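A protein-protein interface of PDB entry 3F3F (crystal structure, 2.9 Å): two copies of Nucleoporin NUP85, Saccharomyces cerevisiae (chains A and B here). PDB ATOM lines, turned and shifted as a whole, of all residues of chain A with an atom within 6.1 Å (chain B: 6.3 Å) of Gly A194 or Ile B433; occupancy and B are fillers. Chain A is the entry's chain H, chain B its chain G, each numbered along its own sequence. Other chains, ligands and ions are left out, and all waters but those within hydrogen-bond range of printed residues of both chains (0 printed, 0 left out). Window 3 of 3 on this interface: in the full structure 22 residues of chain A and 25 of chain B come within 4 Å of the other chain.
Of the printed residues of chain B, Gly A194 touches Ile B433 (3.4 Å). Of the printed residues of chain B, Asp A196 touches Phe B434 (3.5 Å) and Glu B435 (3.0 Å). Leu A368 touches none of the printed residues of chain B. Glu B431 touches none of the printed residues of chain A. Of chain A, only Gly A194 (3.4 Å) and Glu A369 (3.1 Å) come within 4 Å of Ile B433. Of the printed residues of chain A, Glu B435 touches Gln A195 and Asp A196. The nearest residue of chain B that does not touch Gly A194 is Glu B431 (5.1 Å). The nearest residue of chain A that does not touch Ile B433 is Gln A195 (4.02 Å). The nearest printed residue of chain B that does not touch Gln A195 is Ile B433 (4.02 Å).
No position is printed for both chains. Of the 7 pairs that touch across the chains among the printed residues, none has its exchanged pair printed and touching as well.
Of the 9 printed residues of chain A, 4 touch a printed residue of chain B. Printed residues of chain A that touch a printed residue of chain B: Gly A194, Gln A195, Asp A196 and Glu A369. Of the 6 printed residues of chain B, 4 touch a printed residue of chain A. Printed residues of chain B that touch a printed residue of chain A: Asn B432, Ile B433, Phe B434 and Glu B435. Among the printed residues, 7 pairs touch across the chains.
The side-chain amide oxygen (OD1) of Asn B432 sits close to the backbone carbonyl oxygen (O) of Asn B459, 2.8 Å away. OD1 of Asp A196 lies within hydrogen-bond range of N of Leu A368 (3.2 Å).
O of Gly A194 touches CG2 of Ile B433, 3.4 Å away. Gln A195 touches Glu B435 (CB to OE1, 3.3 Å). CD2 of Phe B434 touches OD2 of Asp A196, 3.5 Å away. OD1 of Asn B432 touches OE1 of Glu A369, 3.6 Å away.
N of Ile B433 is in hydrogen-bond range of OE1 of Glu A369 (3.1 Å). The backbone NH of Phe B434 lies within hydrogen-bond range of the side-chain carboxylate of Glu A369, at 3.4 Å. OE1 of Glu B435 is in hydrogen-bond range of N of Asp A196 (3.1 Å).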
ATOM      1  N   MET A 188      11.591  -1.048  33.208  1.00  0.00           N
ATOM      2  CA  MET A 188      11.875  -0.221  32.047  1.00  0.00           C
ATOM      3  C   MET A 188      11.600  -0.797  30.671  1.00  0.00           C
ATOM      4  O   MET A 188      11.483  -0.036  29.717  1.00  0.00           O
ATOM      5  CB  MET A 188      13.322   0.237  32.105  1.00  0.00           C
ATOM      6  CG  MET A 188      13.691   0.881  33.423  1.00  0.00           C
ATOM      7  SD  MET A 188      12.834   2.417  33.636  1.00  0.00           S
ATOM      8  CE  MET A 188      13.584   3.383  32.201  1.00  0.00           C
ATOM      9  N   TYR A 189      11.499  -2.118  30.541  1.00  0.00           N
ATOM     10  CA  TYR A 189      11.261  -2.706  29.212  1.00  0.00           C
ATOM     11  C   TYR A 189      10.227  -3.827  29.129  1.00  0.00           C
ATOM     12  O   TYR A 189       9.807  -4.212  28.029  1.00  0.00           O
ATOM     13  CB  TYR A 189      12.579  -3.225  28.607  1.00  0.00           C
ATOM     14  CG  TYR A 189      13.619  -2.151  28.379  1.00  0.00           C
ATOM     15  CD1 TYR A 189      14.404  -1.679  29.431  1.00  0.00           C
ATOM     16  CD2 TYR A 189      13.754  -1.543  27.139  1.00  0.00           C
ATOM     17  CE1 TYR A 189      15.291  -0.627  29.257  1.00  0.00           C
ATOM     18  CE2 TYR A 189      14.634  -0.490  26.955  1.00  0.00           C
ATOM     19  CZ  TYR A 189      15.398  -0.035  28.021  1.00  0.00           C
ATOM     20  OH  TYR A 189      16.254   1.033  27.866  1.00  0.00           O
ATOM     21  N   LEU A 192       5.653  -1.557  29.724  1.00  0.00           N
ATOM     22  CA  LEU A 192       5.077  -0.602  28.787  1.00  0.00           C
ATOM     23  C   LEU A 192       5.309  -0.933  27.323  1.00  0.00           C
ATOM     24  O   LEU A 192       4.692  -0.329  26.455  1.00  0.00           O
ATOM     25  CB  LEU A 192       5.616   0.795  29.092  1.00  0.00           C
ATOM     26  CG  LEU A 192       5.456   1.169  30.567  1.00  0.00           C
ATOM     27  CD1 LEU A 192       6.075   2.517  30.835  1.00  0.00           C
ATOM     28  CD2 LEU A 192       3.986   1.174  30.926  1.00  0.00           C
ATOM     29  N   ASP A 193       6.189  -1.888  27.050  1.00  0.00           N
ATOM     30  CA  ASP A 193       6.497  -2.287  25.676  1.00  0.00           C
ATOM     31  C   ASP A 193       6.768  -1.110  24.733  1.00  0.00           C
ATOM     32  O   ASP A 193       6.206  -1.040  23.641  1.00  0.00           O
ATOM     33  CB  ASP A 193       5.357  -3.128  25.103  1.00  0.00           C
ATOM     34  CG  ASP A 193       4.931  -4.248  26.036  1.00  0.00           C
ATOM     35  OD1 ASP A 193       5.807  -4.794  26.749  1.00  0.00           O
ATOM     36  OD2 ASP A 193       3.724  -4.590  26.047  1.00  0.00           O
ATOM     37  N   GLY A 194       7.625  -0.188  25.162  1.00  0.00           N
ATOM     38  CA  GLY A 194       7.971   0.962  24.344  1.00  0.00           C
ATOM     39  C   GLY A 194       7.045   2.156  24.462  1.00  0.00           C
ATOM     40  O   GLY A 194       7.353   3.231  23.948  1.00  0.00           O
ATOM     41  N   GLN A 195       5.916   1.981  25.137  1.00  0.00           N
ATOM     42  CA  GLN A 195       4.953   3.062  25.290  1.00  0.00           C
ATOM     43  C   GLN A 195       5.289   3.891  26.505  1.00  0.00           C
ATOM     44  O   GLN A 195       6.332   3.689  27.122  1.00  0.00           O
ATOM     45  CB  GLN A 195       3.549   2.490  25.429  1.00  0.00           C
ATOM     46  CG  GLN A 195       3.247   1.379  24.422  1.00  0.00           C
ATOM     47  CD  GLN A 195       3.332   1.845  22.969  1.00  0.00           C
ATOM     48  OE1 GLN A 195       4.322   2.464  22.553  1.00  0.00           O
ATOM     49  NE2 GLN A 195       2.293   1.540  22.186  1.00  0.00           N
ATOM     50  N   ASP A 196       4.408   4.822  26.851  1.00  0.00           N
ATOM     51  CA  ASP A 196       4.646   5.675  28.009  1.00  0.00           C
ATOM     52  C   ASP A 196       3.797   5.227  29.190  1.00  0.00           C
ATOM     53  O   ASP A 196       2.899   4.404  29.041  1.00  0.00           O
ATOM     54  CB  ASP A 196       4.347   7.143  27.679  1.00  0.00           C
ATOM     55  CG  ASP A 196       5.279   8.108  28.405  1.00  0.00           C
ATOM     56  OD1 ASP A 196       5.376   8.038  29.647  1.00  0.00           O
ATOM     57  OD2 ASP A 196       5.920   8.941  27.733  1.00  0.00           O
ATOM     58  N   LEU A 368       8.445   8.577  30.372  1.00  0.00           N
ATOM     59  CA  LEU A 368       9.758   7.992  30.124  1.00  0.00           C
ATOM     60  C   LEU A 368      10.516   8.725  29.031  1.00  0.00           C
ATOM     61  O   LEU A 368      11.679   8.455  28.782  1.00  0.00           O
ATOM     62  CB  LEU A 368       9.611   6.512  29.763  1.00  0.00           C
ATOM     63  CG  LEU A 368       9.321   5.618  30.971  1.00  0.00           C
ATOM     64  CD1 LEU A 368       9.153   4.192  30.509  1.00  0.00           C
ATOM     65  CD2 LEU A 368      10.466   5.728  31.988  1.00  0.00           C
ATOM     66  N   GLU A 369       9.841   9.652  28.373  1.00  0.00           N
ATOM     67  CA  GLU A 369      10.467  10.442  27.332  1.00  0.00           C
ATOM     68  C   GLU A 369      11.452  11.415  28.006  1.00  0.00           C
ATOM     69  O   GLU A 369      12.318  12.005  27.363  1.00  0.00           O
ATOM     70  CB  GLU A 369       9.385  11.199  26.558  1.00  0.00           C
ATOM     71  CG  GLU A 369       9.891  12.252  25.576  1.00  0.00           C
ATOM     72  CD  GLU A 369      10.700  11.676  24.425  1.00  0.00           C
ATOM     73  OE1 GLU A 369      10.221  10.704  23.806  1.00  0.00           O
ATOM     74  OE2 GLU A 369      11.801  12.202  24.131  1.00  0.00           O
ATOM     75  N   GLU B 431      13.620   7.653  18.583  1.00  0.00           N
ATOM     76  CA  GLU B 431      12.230   7.920  18.242  1.00  0.00           C
ATOM     77  C   GLU B 431      11.434   8.500  19.401  1.00  0.00           C
ATOM     78  O   GLU B 431      11.853   8.440  20.561  1.00  0.00           O
ATOM     79  CB  GLU B 431      11.544   6.650  17.747  1.00  0.00           C
ATOM     80  CG  GLU B 431      11.340   5.588  18.826  1.00  0.00           C
ATOM     81  CD  GLU B 431      10.102   4.727  18.569  1.00  0.00           C
ATOM     82  OE1 GLU B 431      10.053   4.038  17.519  1.00  0.00           O
ATOM     83  OE2 GLU B 431       9.177   4.746  19.419  1.00  0.00           O
ATOM     84  N   ASN B 432      10.281   9.064  19.066  1.00  0.00           N
ATOM     85  CA  ASN B 432       9.390   9.659  20.048  1.00  0.00           C
ATOM     86  C   ASN B 432       8.683   8.557  20.860  1.00  0.00           C
ATOM     87  O   ASN B 432       7.761   7.904  20.379  1.00  0.00           O
ATOM     88  CB  ASN B 432       8.381  10.548  19.311  1.00  0.00           C
ATOM     89  CG  ASN B 432       7.485  11.333  20.247  1.00  0.00           C
ATOM     90  OD1 ASN B 432       7.941  11.861  21.260  1.00  0.00           O
ATOM     91  ND2 ASN B 432       6.203  11.431  19.901  1.00  0.00           N
ATOM     92  N   ILE B 433       9.142   8.350  22.090  1.00  0.00           N
ATOM     93  CA  ILE B 433       8.578   7.335  22.984  1.00  0.00           C
ATOM     94  C   ILE B 433       7.315   7.863  23.661  1.00  0.00           C
ATOM     95  O   ILE B 433       6.503   7.083  24.160  1.00  0.00           O
ATOM     96  CB  ILE B 433       9.604   6.932  24.101  1.00  0.00           C
ATOM     97  CG1 ILE B 433      10.840   6.265  23.476  1.00  0.00           C
ATOM     98  CG2 ILE B 433       8.942   6.011  25.124  1.00  0.00           C
ATOM     99  CD1 ILE B 433      12.005   6.050  24.450  1.00  0.00           C
ATOM    100  N   PHE B 434       7.154   9.188  23.658  1.00  0.00           N
ATOM    101  CA  PHE B 434       6.016   9.850  24.302  1.00  0.00           C
ATOM    102  C   PHE B 434       4.622   9.412  23.867  1.00  0.00           C
ATOM    103  O   PHE B 434       4.376   9.057  22.706  1.00  0.00           O
ATOM    104  CB  PHE B 434       6.133  11.380  24.170  1.00  0.00           C
ATOM    105  CG  PHE B 434       5.098  12.156  24.974  1.00  0.00           C
ATOM    106  CD1 PHE B 434       4.138  12.939  24.337  1.00  0.00           C
ATOM    107  CD2 PHE B 434       5.092  12.109  26.365  1.00  0.00           C
ATOM    108  CE1 PHE B 434       3.195  13.662  25.069  1.00  0.00           C
ATOM    109  CE2 PHE B 434       4.148  12.832  27.105  1.00  0.00           C
ATOM    110  CZ  PHE B 434       3.202  13.607  26.452  1.00  0.00           C
ATOM    111  N   GLU B 435       3.740   9.457  24.870  1.00  0.00           N
ATOM    112  CA  GLU B 435       2.316   9.112  24.834  1.00  0.00           C
ATOM    113  C   GLU B 435       1.771   9.603  26.195  1.00  0.00           C
ATOM    114  O   GLU B 435       1.930   8.932  27.224  1.00  0.00           O
ATOM    115  CB  GLU B 435       2.138   7.593  24.709  1.00  0.00           C
ATOM    116  CG  GLU B 435       0.721   7.108  24.969  1.00  0.00           C
ATOM    117  CD  GLU B 435       0.631   5.598  25.080  1.00  0.00           C
ATOM    118  OE1 GLU B 435       1.469   5.007  25.797  1.00  0.00           O
ATOM    119  OE2 GLU B 435      -0.282   5.004  24.462  1.00  0.00           O
ATOM    120  N   ASN B 459       6.673  15.859  21.644  1.00  0.00           N
ATOM    121  CA  ASN B 459       7.018  15.242  20.374  1.00  0.00           C
ATOM    122  C   ASN B 459       8.438  14.696  20.477  1.00  0.00           C
ATOM    123  O   ASN B 459       8.927  14.439  21.575  1.00  0.00           O
ATOM    124  CB  ASN B 459       6.902  16.268  19.259  1.00  0.00           C
ATOM    125  CG  ASN B 459       5.511  16.876  19.187  1.00  0.00           C
ATOM    126  OD1 ASN B 459       4.519  16.159  19.078  1.00  0.00           O
ATOM    127  ND2 ASN B 459       5.432  18.200  19.250  1.00  0.00           N
